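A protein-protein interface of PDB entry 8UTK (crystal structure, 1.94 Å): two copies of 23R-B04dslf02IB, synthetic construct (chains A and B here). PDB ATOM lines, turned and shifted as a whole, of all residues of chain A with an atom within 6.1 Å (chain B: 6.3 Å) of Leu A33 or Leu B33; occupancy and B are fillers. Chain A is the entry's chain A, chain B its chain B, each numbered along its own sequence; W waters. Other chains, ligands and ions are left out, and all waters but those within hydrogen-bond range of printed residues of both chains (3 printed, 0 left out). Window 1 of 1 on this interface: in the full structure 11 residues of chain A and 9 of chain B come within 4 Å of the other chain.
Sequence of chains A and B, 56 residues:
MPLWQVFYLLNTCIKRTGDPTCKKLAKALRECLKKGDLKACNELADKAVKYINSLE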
ATOM      1  N   LEU A   3      -4.610 -28.302  -9.809  1.00  0.00           N
ATOM      2  CA  LEU A   3      -5.790 -27.596  -9.310  1.00  0.00           C
ATOM      3  C   LEU A   3      -7.048 -28.462  -9.369  1.00  0.00           C
ATOM      4  O   LEU A   3      -7.830 -28.493  -8.416  1.00  0.00           O
ATOM      5  CB  LEU A   3      -5.993 -26.292 -10.085  1.00  0.00           C
ATOM      6  CG  LEU A   3      -6.962 -25.305  -9.417  1.00  0.00           C
ATOM      7  CD1 LEU A   3      -6.636 -25.165  -7.927  1.00  0.00           C
ATOM      8  CD2 LEU A   3      -6.941 -23.941 -10.101  1.00  0.00           C
ATOM      9  N   TRP A   4      -7.269 -29.172 -10.480  1.00  0.00           N
ATOM     10  CA  TRP A   4      -8.509 -29.940 -10.601  1.00  0.00           C
ATOM     11  C   TRP A   4      -8.552 -31.095  -9.604  1.00  0.00           C
ATOM     12  O   TRP A   4      -9.634 -31.479  -9.152  1.00  0.00           O
ATOM     13  CB  TRP A   4      -8.677 -30.463 -12.028  1.00  0.00           C
ATOM     14  CG  TRP A   4      -7.569 -31.380 -12.389  1.00  0.00           C
ATOM     15  CD1 TRP A   4      -6.379 -31.046 -12.975  1.00  0.00           C
ATOM     16  CD2 TRP A   4      -7.514 -32.785 -12.133  1.00  0.00           C
ATOM     17  NE1 TRP A   4      -5.596 -32.168 -13.117  1.00  0.00           N
ATOM     18  CE2 TRP A   4      -6.269 -33.249 -12.608  1.00  0.00           C
ATOM     19  CE3 TRP A   4      -8.403 -33.700 -11.557  1.00  0.00           C
ATOM     20  CZ2 TRP A   4      -5.892 -34.589 -12.528  1.00  0.00           C
ATOM     21  CZ3 TRP A   4      -8.023 -35.031 -11.473  1.00  0.00           C
ATOM     22  CH2 TRP A   4      -6.783 -35.463 -11.958  1.00  0.00           C
ATOM     23  N   PHE A   7      -9.643 -29.772  -6.191  1.00  0.00           N
ATOM     24  CA  PHE A   7     -11.086 -29.642  -6.108  1.00  0.00           C
ATOM     25  C   PHE A   7     -11.773 -30.986  -6.099  1.00  0.00           C
ATOM     26  O   PHE A   7     -12.787 -31.144  -5.407  1.00  0.00           O
ATOM     27  CB  PHE A   7     -11.594 -28.750  -7.225  1.00  0.00           C
ATOM     28  CG  PHE A   7     -11.583 -27.316  -6.823  1.00  0.00           C
ATOM     29  CD1 PHE A   7     -12.590 -26.810  -6.025  1.00  0.00           C
ATOM     30  CD2 PHE A   7     -10.528 -26.507  -7.143  1.00  0.00           C
ATOM     31  CE1 PHE A   7     -12.563 -25.489  -5.602  1.00  0.00           C
ATOM     32  CE2 PHE A   7     -10.490 -25.179  -6.718  1.00  0.00           C
ATOM     33  CZ  PHE A   7     -11.508 -24.676  -5.951  1.00  0.00           C
ATOM     34  N   ASN A  11     -14.266 -31.644  -3.168  1.00  0.00           N
ATOM     35  CA  ASN A  11     -15.657 -31.888  -3.515  1.00  0.00           C
ATOM     36  C   ASN A  11     -16.118 -33.268  -3.066  1.00  0.00           C
ATOM     37  O   ASN A  11     -17.283 -33.430  -2.702  1.00  0.00           O
ATOM     38  CB  ASN A  11     -15.859 -31.709  -5.008  1.00  0.00           C
ATOM     39  CG  ASN A  11     -15.742 -30.259  -5.412  1.00  0.00           C
ATOM     40  OD1 ASN A  11     -15.792 -29.384  -4.563  1.00  0.00           O
ATOM     41  ND2 ASN A  11     -15.582 -29.999  -6.695  1.00  0.00           N
ATOM     42  N   ALA A  28     -12.909 -20.761  -0.036  1.00  0.00           N
ATOM     43  CA  ALA A  28     -11.763 -19.866   0.074  1.00  0.00           C
ATOM     44  C   ALA A  28     -10.854 -19.969  -1.140  1.00  0.00           C
ATOM     45  O   ALA A  28     -10.333 -18.954  -1.626  1.00  0.00           O
ATOM     46  CB  ALA A  28     -10.976 -20.192   1.344  1.00  0.00           C
ATOM     47  N   LEU A  29     -10.623 -21.192  -1.633  1.00  0.00           N
ATOM     48  CA  LEU A  29      -9.765 -21.341  -2.803  1.00  0.00           C
ATOM     49  C   LEU A  29     -10.407 -20.708  -4.034  1.00  0.00           C
ATOM     50  O   LEU A  29      -9.709 -20.107  -4.857  1.00  0.00           O
ATOM     51  CB  LEU A  29      -9.461 -22.821  -3.030  1.00  0.00           C
ATOM     52  CG  LEU A  29      -8.474 -23.213  -4.123  1.00  0.00           C
ATOM     53  CD1 LEU A  29      -7.177 -22.418  -3.984  1.00  0.00           C
ATOM     54  CD2 LEU A  29      -8.201 -24.735  -4.058  1.00  0.00           C
ATOM     55  N   ARG A  30     -11.736 -20.846  -4.182  1.00  0.00           N
ATOM     56  CA  ARG A  30     -12.462 -20.169  -5.267  1.00  0.00           C
ATOM     57  C   ARG A  30     -12.382 -18.649  -5.136  1.00  0.00           C
ATOM     58  O   ARG A  30     -12.225 -17.936  -6.138  1.00  0.00           O
ATOM     59  CB  ARG A  30     -13.939 -20.594  -5.271  1.00  0.00           C
ATOM     60  CG  ARG A  30     -14.275 -21.899  -6.000  1.00  0.00           C
ATOM     61  CD  ARG A  30     -15.627 -22.455  -5.507  1.00  0.00           C
ATOM     62  NE  ARG A  30     -16.672 -21.431  -5.460  1.00  0.00           N
ATOM     63  CZ  ARG A  30     -17.630 -21.382  -4.541  1.00  0.00           C
ATOM     64  NH1 ARG A  30     -17.704 -22.280  -3.571  1.00  0.00           N
ATOM     65  NH2 ARG A  30     -18.534 -20.403  -4.590  1.00  0.00           N
ATOM     66  N   GLU A  31     -12.532 -18.122  -3.917  1.00  0.00           N
ATOM     67  CA  GLU A  31     -12.382 -16.679  -3.746  1.00  0.00           C
ATOM     68  C   GLU A  31     -10.944 -16.248  -3.991  1.00  0.00           C
ATOM     69  O   GLU A  31     -10.698 -15.171  -4.546  1.00  0.00           O
ATOM     70  CB  GLU A  31     -12.833 -16.256  -2.354  1.00  0.00           C
ATOM     71  CG  GLU A  31     -14.319 -16.432  -2.137  1.00  0.00           C
ATOM     72  CD  GLU A  31     -14.732 -16.159  -0.703  1.00  0.00           C
ATOM     73  OE1 GLU A  31     -13.850 -16.152   0.185  1.00  0.00           O
ATOM     74  OE2 GLU A  31     -15.943 -15.951  -0.466  1.00  0.00           O
ATOM     75  N   CYS A  32      -9.978 -17.082  -3.589  1.00  0.00           N
ATOM     76  CA  CYS A  32      -8.581 -16.773  -3.864  1.00  0.00           C
ATOM     77  C   CYS A  32      -8.307 -16.733  -5.368  1.00  0.00           C
ATOM     78  O   CYS A  32      -7.588 -15.852  -5.854  1.00  0.00           O
ATOM     79  CB  CYS A  32      -7.676 -17.793  -3.180  1.00  0.00           C
ATOM     80  SG  CYS A  32      -5.950 -17.348  -3.362  1.00  0.00           S
ATOM     81  N   LEU A  33      -8.848 -17.689  -6.122  1.00  0.00           N
ATOM     82  CA  LEU A  33      -8.636 -17.687  -7.568  1.00  0.00           C
ATOM     83  C   LEU A  33      -9.261 -16.457  -8.208  1.00  0.00           C
ATOM     84  O   LEU A  33      -8.801 -15.995  -9.256  1.00  0.00           O
ATOM     85  CB  LEU A  33      -9.227 -18.951  -8.191  1.00  0.00           C
ATOM     86  CG  LEU A  33      -8.487 -20.250  -7.879  1.00  0.00           C
ATOM     87  CD1 LEU A  33      -9.333 -21.449  -8.273  1.00  0.00           C
ATOM     88  CD2 LEU A  33      -7.176 -20.258  -8.604  1.00  0.00           C
ATOM     89  N   LYS A  34     -10.315 -15.923  -7.599  1.00  0.00           N
ATOM     90  CA  LYS A  34     -10.965 -14.748  -8.160  1.00  0.00           C
ATOM     91  C   LYS A  34     -10.106 -13.513  -7.941  1.00  0.00           C
ATOM     92  O   LYS A  34      -9.915 -12.714  -8.863  1.00  0.00           O
ATOM     93  CB  LYS A  34     -12.351 -14.581  -7.534  1.00  0.00           C
ATOM     94  CG  LYS A  34     -13.199 -13.447  -8.104  1.00  0.00           C
ATOM     95  CD  LYS A  34     -14.578 -13.422  -7.439  1.00  0.00           C
ATOM     96  CE  LYS A  34     -15.467 -12.315  -8.010  1.00  0.00           C
ATOM     97  NZ  LYS A  34     -16.718 -12.151  -7.223  1.00  0.00           N
ATOM     98  N   LYS A  35      -9.550 -13.362  -6.734  1.00  0.00           N
ATOM     99  CA  LYS A  35      -8.642 -12.255  -6.443  1.00  0.00           C
ATOM    100  C   LYS A  35      -7.344 -12.358  -7.237  1.00  0.00           C
ATOM    101  O   LYS A  35      -6.738 -11.332  -7.562  1.00  0.00           O
ATOM    102  CB  LYS A  35      -8.342 -12.197  -4.940  1.00  0.00           C
ATOM    103  CG  LYS A  35      -9.499 -11.658  -4.089  1.00  0.00           C
ATOM    104  CD  LYS A  35      -9.237 -11.814  -2.584  1.00  0.00           C
ATOM    105  CE  LYS A  35      -9.292 -13.284  -2.162  1.00  0.00           C
ATOM    106  NZ  LYS A  35      -9.119 -13.520  -0.697  1.00  0.00           N
ATOM    107  N   GLY A  36      -6.891 -13.570  -7.542  1.00  0.00           N
ATOM    108  CA  GLY A  36      -5.761 -13.743  -8.433  1.00  0.00           C
ATOM    109  C   GLY A  36      -4.392 -13.772  -7.792  1.00  0.00           C
ATOM    110  O   GLY A  36      -3.389 -13.612  -8.503  1.00  0.00           O
ATOM    111  N   ASP A  37      -4.303 -13.967  -6.476  1.00  0.00           N
ATOM    112  CA  ASP A  37      -3.006 -14.136  -5.816  1.00  0.00           C
ATOM    113  C   ASP A  37      -2.656 -15.622  -5.834  1.00  0.00           C
ATOM    114  O   ASP A  37      -2.885 -16.357  -4.872  1.00  0.00           O
ATOM    115  CB  ASP A  37      -3.055 -13.581  -4.399  1.00  0.00           C
ATOM    116  CG  ASP A  37      -1.704 -13.647  -3.686  1.00  0.00           C
ATOM    117  OD1 ASP A  37      -0.700 -14.103  -4.292  1.00  0.00           O
ATOM    118  OD2 ASP A  37      -1.655 -13.236  -2.505  1.00  0.00           O
ATOM    119  N   LEU A  38      -2.064 -16.067  -6.952  1.00  0.00           N
ATOM    120  CA  LEU A  38      -1.949 -17.504  -7.190  1.00  0.00           C
ATOM    121  C   LEU A  38      -0.913 -18.156  -6.282  1.00  0.00           C
ATOM    122  O   LEU A  38      -1.059 -19.331  -5.930  1.00  0.00           O
ATOM    123  CB  LEU A  38      -1.637 -17.782  -8.663  1.00  0.00           C
ATOM    124  CG  LEU A  38      -2.763 -17.422  -9.644  1.00  0.00           C
ATOM    125  CD1 LEU A  38      -2.439 -17.942 -11.025  1.00  0.00           C
ATOM    126  CD2 LEU A  38      -4.114 -17.955  -9.184  1.00  0.00           C
ATOM    127  N   CYS A  41      -3.160 -18.769  -3.392  1.00  0.00           N
ATOM    128  CA  CYS A  41      -4.081 -19.859  -3.695  1.00  0.00           C
ATOM    129  C   CYS A  41      -3.369 -21.198  -3.671  1.00  0.00           C
ATOM    130  O   CYS A  41      -3.938 -22.207  -3.241  1.00  0.00           O
ATOM    131  CB  CYS A  41      -4.743 -19.650  -5.054  1.00  0.00           C
ATOM    132  SG  CYS A  41      -5.448 -18.011  -5.277  1.00  0.00           S
ATOM    133  N   LEU B   3      -4.610 -25.989 -15.171  1.00  0.00           N
ATOM    134  CA  LEU B   3      -5.498 -24.888 -14.810  1.00  0.00           C
ATOM    135  C   LEU B   3      -4.757 -23.751 -14.113  1.00  0.00           C
ATOM    136  O   LEU B   3      -5.156 -22.587 -14.263  1.00  0.00           O
ATOM    137  CB  LEU B   3      -6.642 -25.398 -13.937  1.00  0.00           C
ATOM    138  CG  LEU B   3      -7.712 -26.206 -14.658  1.00  0.00           C
ATOM    139  CD1 LEU B   3      -8.703 -26.742 -13.633  1.00  0.00           C
ATOM    140  CD2 LEU B   3      -8.425 -25.351 -15.681  1.00  0.00           C
ATOM    141  N   TRP B   4      -3.693 -24.043 -13.350  1.00  0.00           N
ATOM    142  CA  TRP B   4      -2.907 -22.957 -12.762  1.00  0.00           C
ATOM    143  C   TRP B   4      -2.434 -21.982 -13.840  1.00  0.00           C
ATOM    144  O   TRP B   4      -2.527 -20.754 -13.687  1.00  0.00           O
ATOM    145  CB  TRP B   4      -1.695 -23.494 -11.994  1.00  0.00           C
ATOM    146  CG  TRP B   4      -1.983 -24.211 -10.708  1.00  0.00           C
ATOM    147  CD1 TRP B   4      -1.698 -25.516 -10.426  1.00  0.00           C
ATOM    148  CD2 TRP B   4      -2.569 -23.662  -9.519  1.00  0.00           C
ATOM    149  NE1 TRP B   4      -2.080 -25.817  -9.143  1.00  0.00           N
ATOM    150  CE2 TRP B   4      -2.621 -24.700  -8.564  1.00  0.00           C
ATOM    151  CE3 TRP B   4      -3.075 -22.401  -9.173  1.00  0.00           C
ATOM    152  CZ2 TRP B   4      -3.152 -24.517  -7.285  1.00  0.00           C
ATOM    153  CZ3 TRP B   4      -3.598 -22.219  -7.900  1.00  0.00           C
ATOM    154  CH2 TRP B   4      -3.629 -23.273  -6.968  1.00  0.00           C
ATOM    155  N   PHE B   7      -5.481 -19.942 -15.210  1.00  0.00           N
ATOM    156  CA  PHE B   7      -5.936 -18.863 -14.340  1.00  0.00           C
ATOM    157  C   PHE B   7      -4.942 -17.708 -14.352  1.00  0.00           C
ATOM    158  O   PHE B   7      -5.340 -16.538 -14.356  1.00  0.00           O
ATOM    159  CB  PHE B   7      -6.158 -19.380 -12.916  1.00  0.00           C
ATOM    160  CG  PHE B   7      -7.558 -19.897 -12.673  1.00  0.00           C
ATOM    161  CD1 PHE B   7      -8.622 -19.017 -12.578  1.00  0.00           C
ATOM    162  CD2 PHE B   7      -7.806 -21.247 -12.549  1.00  0.00           C
ATOM    163  CE1 PHE B   7      -9.915 -19.475 -12.359  1.00  0.00           C
ATOM    164  CE2 PHE B   7      -9.099 -21.718 -12.334  1.00  0.00           C
ATOM    165  CZ  PHE B   7     -10.153 -20.830 -12.238  1.00  0.00           C
ATOM    166  N   ASN B  11      -6.163 -14.138 -15.308  1.00  0.00           N
ATOM    167  CA  ASN B  11      -6.116 -13.061 -14.327  1.00  0.00           C
ATOM    168  C   ASN B  11      -5.171 -11.956 -14.772  1.00  0.00           C
ATOM    169  O   ASN B  11      -5.442 -10.777 -14.519  1.00  0.00           O
ATOM    170  CB  ASN B  11      -5.733 -13.594 -12.948  1.00  0.00           C
ATOM    171  CG  ASN B  11      -6.867 -14.375 -12.297  1.00  0.00           C
ATOM    172  OD1 ASN B  11      -8.024 -14.246 -12.694  1.00  0.00           O
ATOM    173  ND2 ASN B  11      -6.540 -15.188 -11.305  1.00  0.00           N
ATOM    174  N   ALA B  28     -16.443 -18.853 -15.330  1.00  0.00           N
ATOM    175  CA  ALA B  28     -16.920 -20.167 -15.744  1.00  0.00           C
ATOM    176  C   ALA B  28     -15.992 -21.278 -15.270  1.00  0.00           C
ATOM    177  O   ALA B  28     -16.452 -22.385 -14.951  1.00  0.00           O
ATOM    178  CB  ALA B  28     -17.073 -20.200 -17.265  1.00  0.00           C
ATOM    179  N   LEU B  29     -14.685 -21.012 -15.211  1.00  0.00           N
ATOM    180  CA  LEU B  29     -13.778 -22.013 -14.667  1.00  0.00           C
ATOM    181  C   LEU B  29     -13.986 -22.194 -13.171  1.00  0.00           C
ATOM    182  O   LEU B  29     -13.940 -23.321 -12.673  1.00  0.00           O
ATOM    183  CB  LEU B  29     -12.334 -21.645 -14.962  1.00  0.00           C
ATOM    184  CG  LEU B  29     -11.821 -22.193 -16.288  1.00  0.00           C
ATOM    185  CD1 LEU B  29     -10.449 -21.635 -16.550  1.00  0.00           C
ATOM    186  CD2 LEU B  29     -11.777 -23.703 -16.244  1.00  0.00           C
ATOM    187  N   ARG B  30     -14.210 -21.103 -12.428  1.00  0.00           N
ATOM    188  CA  ARG B  30     -14.463 -21.259 -10.996  1.00  0.00           C
ATOM    189  C   ARG B  30     -15.717 -22.099 -10.745  1.00  0.00           C
ATOM    190  O   ARG B  30     -15.747 -22.930  -9.830  1.00  0.00           O
ATOM    191  CB  ARG B  30     -14.577 -19.890 -10.323  1.00  0.00           C
ATOM    192  CG  ARG B  30     -13.221 -19.108 -10.342  1.00  0.00           C
ATOM    193  CD  ARG B  30     -13.202 -17.915  -9.401  1.00  0.00           C
ATOM    194  NE  ARG B  30     -14.251 -16.955  -9.716  1.00  0.00           N
ATOM    195  CZ  ARG B  30     -14.164 -16.038 -10.671  1.00  0.00           C
ATOM    196  NH1 ARG B  30     -13.068 -15.909 -11.413  1.00  0.00           N
ATOM    197  NH2 ARG B  30     -15.194 -15.227 -10.884  1.00  0.00           N
ATOM    198  N   GLU B  31     -16.748 -21.920 -11.577  1.00  0.00           N
ATOM    199  CA  GLU B  31     -17.979 -22.693 -11.435  1.00  0.00           C
ATOM    200  C   GLU B  31     -17.763 -24.171 -11.757  1.00  0.00           C
ATOM    201  O   GLU B  31     -18.158 -25.039 -10.976  1.00  0.00           O
ATOM    202  CB  GLU B  31     -19.070 -22.102 -12.330  1.00  0.00           C
ATOM    203  CG  GLU B  31     -20.442 -22.771 -12.158  1.00  0.00           C
ATOM    204  CD  GLU B  31     -21.232 -22.217 -10.977  1.00  0.00           C
ATOM    205  OE1 GLU B  31     -20.614 -21.876  -9.944  1.00  0.00           O
ATOM    206  OE2 GLU B  31     -22.476 -22.116 -11.087  1.00  0.00           O
ATOM    207  N   CYS B  32     -17.153 -24.490 -12.909  1.00  0.00           N
ATOM    208  CA  CYS B  32     -16.903 -25.896 -13.248  1.00  0.00           C
ATOM    209  C   CYS B  32     -16.069 -26.583 -12.178  1.00  0.00           C
ATOM    210  O   CYS B  32     -16.251 -27.777 -11.910  1.00  0.00           O
ATOM    211  CB  CYS B  32     -16.222 -26.025 -14.626  1.00  0.00           C
ATOM    212  SG  CYS B  32     -14.437 -25.576 -14.739  1.00  0.00           S
ATOM    213  N   LEU B  33     -15.145 -25.852 -11.551  1.00  0.00           N
ATOM    214  CA  LEU B  33     -14.430 -26.398 -10.396  1.00  0.00           C
ATOM    215  C   LEU B  33     -15.368 -26.615  -9.203  1.00  0.00           C
ATOM    216  O   LEU B  33     -15.304 -27.657  -8.539  1.00  0.00           O
ATOM    217  CB  LEU B  33     -13.264 -25.477  -9.995  1.00  0.00           C
ATOM    218  CG  LEU B  33     -12.012 -25.419 -10.875  1.00  0.00           C
ATOM    219  CD1 LEU B  33     -11.064 -24.316 -10.398  1.00  0.00           C
ATOM    220  CD2 LEU B  33     -11.304 -26.768 -10.888  1.00  0.00           C
ATOM    221  N   LYS B  34     -16.229 -25.631  -8.907  1.00  0.00           N
ATOM    222  CA  LYS B  34     -17.158 -25.721  -7.783  1.00  0.00           C
ATOM    223  C   LYS B  34     -18.097 -26.916  -7.931  1.00  0.00           C
ATOM    224  O   LYS B  34     -18.352 -27.646  -6.965  1.00  0.00           O
ATOM    225  CB  LYS B  34     -17.956 -24.418  -7.692  1.00  0.00           C
ATOM    226  CG  LYS B  34     -19.139 -24.446  -6.751  1.00  0.00           C
ATOM    227  CD  LYS B  34     -20.004 -23.187  -6.920  1.00  0.00           C
ATOM    228  CE  LYS B  34     -20.991 -23.020  -5.766  1.00  0.00           C
ATOM    229  NZ  LYS B  34     -21.728 -21.715  -5.773  1.00  0.00           N
ATOM    230  N   LYS B  35     -18.600 -27.138  -9.141  1.00  0.00           N
ATOM    231  CA  LYS B  35     -19.553 -28.198  -9.432  1.00  0.00           C
ATOM    232  C   LYS B  35     -18.890 -29.498  -9.878  1.00  0.00           C
ATOM    233  O   LYS B  35     -19.596 -30.468 -10.172  1.00  0.00           O
ATOM    234  CB  LYS B  35     -20.535 -27.715 -10.502  1.00  0.00           C
ATOM    235  CG  LYS B  35     -21.316 -26.486 -10.058  1.00  0.00           C
ATOM    236  CD  LYS B  35     -22.431 -26.129 -11.031  1.00  0.00           C
ATOM    237  CE  LYS B  35     -23.322 -25.040 -10.438  1.00  0.00           C
ATOM    238  NZ  LYS B  35     -23.742 -25.325  -9.029  1.00  0.00           N
ATOM    239  N   GLY B  36     -17.562 -29.548  -9.930  1.00  0.00           N
ATOM    240  CA  GLY B  36     -16.877 -30.772 -10.307  1.00  0.00           C
ATOM    241  C   GLY B  36     -17.149 -31.259 -11.713  1.00  0.00           C
ATOM    242  O   GLY B  36     -17.066 -32.466 -11.962  1.00  0.00           O
ATOM    243  N   ASP B  37     -17.478 -30.358 -12.643  1.00  0.00           N
ATOM    244  CA  ASP B  37     -17.658 -30.734 -14.046  1.00  0.00           C
ATOM    245  C   ASP B  37     -16.321 -30.577 -14.768  1.00  0.00           C
ATOM    246  O   ASP B  37     -16.056 -29.582 -15.446  1.00  0.00           O
ATOM    247  CB  ASP B  37     -18.746 -29.895 -14.702  1.00  0.00           C
ATOM    248  CG  ASP B  37     -19.053 -30.348 -16.130  1.00  0.00           C
ATOM    249  OD1 ASP B  37     -18.444 -31.337 -16.604  1.00  0.00           O
ATOM    250  OD2 ASP B  37     -19.916 -29.714 -16.776  1.00  0.00           O
ATOM    251  N   LEU B  38     -15.474 -31.603 -14.635  1.00  0.00           N
ATOM    252  CA  LEU B  38     -14.127 -31.532 -15.194  1.00  0.00           C
ATOM    253  C   LEU B  38     -14.120 -31.595 -16.716  1.00  0.00           C
ATOM    254  O   LEU B  38     -13.163 -31.122 -17.335  1.00  0.00           O
ATOM    255  CB  LEU B  38     -13.251 -32.644 -14.611  1.00  0.00           C
ATOM    256  CG  LEU B  38     -12.921 -32.564 -13.112  1.00  0.00           C
ATOM    257  CD1 LEU B  38     -11.838 -33.578 -12.745  1.00  0.00           C
ATOM    258  CD2 LEU B  38     -12.512 -31.151 -12.684  1.00  0.00           C
ATOM    259  N   CYS B  41     -14.487 -27.976 -17.504  1.00  0.00           N
ATOM    260  CA  CYS B  41     -13.234 -27.300 -17.186  1.00  0.00           C
ATOM    261  C   CYS B  41     -12.235 -27.444 -18.326  1.00  0.00           C
ATOM    262  O   CYS B  41     -11.590 -26.468 -18.724  1.00  0.00           O
ATOM    263  CB  CYS B  41     -12.636 -27.851 -15.893  1.00  0.00           C
ATOM    264  SG  CYS B  41     -13.357 -27.271 -14.334  1.00  0.00           S
HETATM  265  O   HOH W   1      -3.634 -27.549 -12.800  1.00  0.00           O
HETATM  266  O   HOH W   2     -10.174 -16.018 -11.410  1.00  0.00           O
HETATM  267  O   HOH W   3     -17.652 -27.259  -4.613  1.00  0.00           O
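O of Phe A7 sits close to ND2 of Asn A11 (3.3 Å).
The side-chain sulfur (SG) of Cys A32 is disulfide-bonded to the side-chain sulfur (SG) of Cys A41, 2.1 Å away.
The backbone NH of Leu A33 sits at hydrogen-bond distance from the side-chain sulfur of Cys A41, 3.5 Å away.
The side-chain sulfur (SG) of Cys B41 sits at hydrogen-bond distance from the backbone NH (N) of Leu B33, 3.6 Å away.
The side-chain sulfur (SG) of Cys B32 is disulfide-bonded to the side-chain sulfur (SG) of Cys B41 (2.1 Å).
Water W3 lies within hydrogen-bond range of the backbone carbonyl oxygen of Lys B34 and the side-chain amide oxygen of Asn A11.
Water W2 lies within hydrogen-bond range of the backbone carbonyl oxygen (O) of Leu A33, the guanidinium group (NH1) of Arg B30 and the side-chain amide oxygen (OD1) of Asn B11.
Water W1 bridges N of Leu B3 and N of Leu A3.
Printed residues of chain B that touch a printed residue of chain A: Trp B4, Phe B7, Asn B11, Arg B30, Leu B33, Lys B34, Gly B36 and Leu B38.
Along chain B the printed residues that touch a printed residue of chain A span positions 4 to 38.
Of the 16 printed residues of chain A, 10 touch a printed residue of chain B.
Among the printed residues, 15 pairs touch across the chains.
Among the printed residues, no Asp or Glu carboxylate lies within 4 Å of a Lys or Arg side-chain nitrogen of the other chain.
Trp A4 touches Leu B38, and with the chains exchanged Leu A38 touches Trp B4.
Asn A11 touches Gly B36, and with the chains exchanged Gly A36 touches Asn B11.
Arg A30 touches its own counterpart, Arg B30.
Arg A30 touches Lys B34, and with the chains exchanged Lys A34 touches Arg B30.
Of the 15 pairs that touch across the chains among the printed residues, 10 have their exchanged pair printed and touching as well.
O of Leu B33 sits at hydrogen-bond distance from ND2 of Asn A11 (3.0 Å).
O of Leu A33 lies within hydrogen-bond range of ND2 of Asn B11 (3.2 Å).
Among the printed residues, pairs that only touch across the chains: Gly A36 with Asn B11 (3.3 Å), Arg A30 with Arg B30 (3.4 Å), Leu A3 with Trp B4 (3.6 Å), Trp A4 with Leu B38 (3.6 Å), Asn A11 with Lys B34 (3.6 Å), Arg A30 with Lys B34 (3.6 Å), Leu A3 with Phe B7 (3.7 Å), Lys A34 with Arg B30 (3.7 Å), Phe A7 with Leu B33 (3.8 Å), Asn A11 with Gly B36 (3.8 Å), Leu A38 with Trp B4 (3.9 Å), Cys A41 with Trp B4 (3.9 Å) and Leu A33 with Leu B33 (3.97 Å).
Printed residues of chain B within 4 Å of Leu A3: Trp B4 (3.6 Å) and Phe B7 (3.7 Å).
Of the printed residues of chain B, Trp A4 touches Leu B38 (3.6 Å).
Leu A33 touches just these residues of chain B: Asn B11 and Leu B33.
Of the printed residues of chain A, Phe B7 touches Leu A3 (3.7 Å).
Of chain A, only Phe A7, Asn A11 and Leu A33 come within 4 Å of Leu B33.
Of the printed residues of chain A, Gly B36 touches Asn A11.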
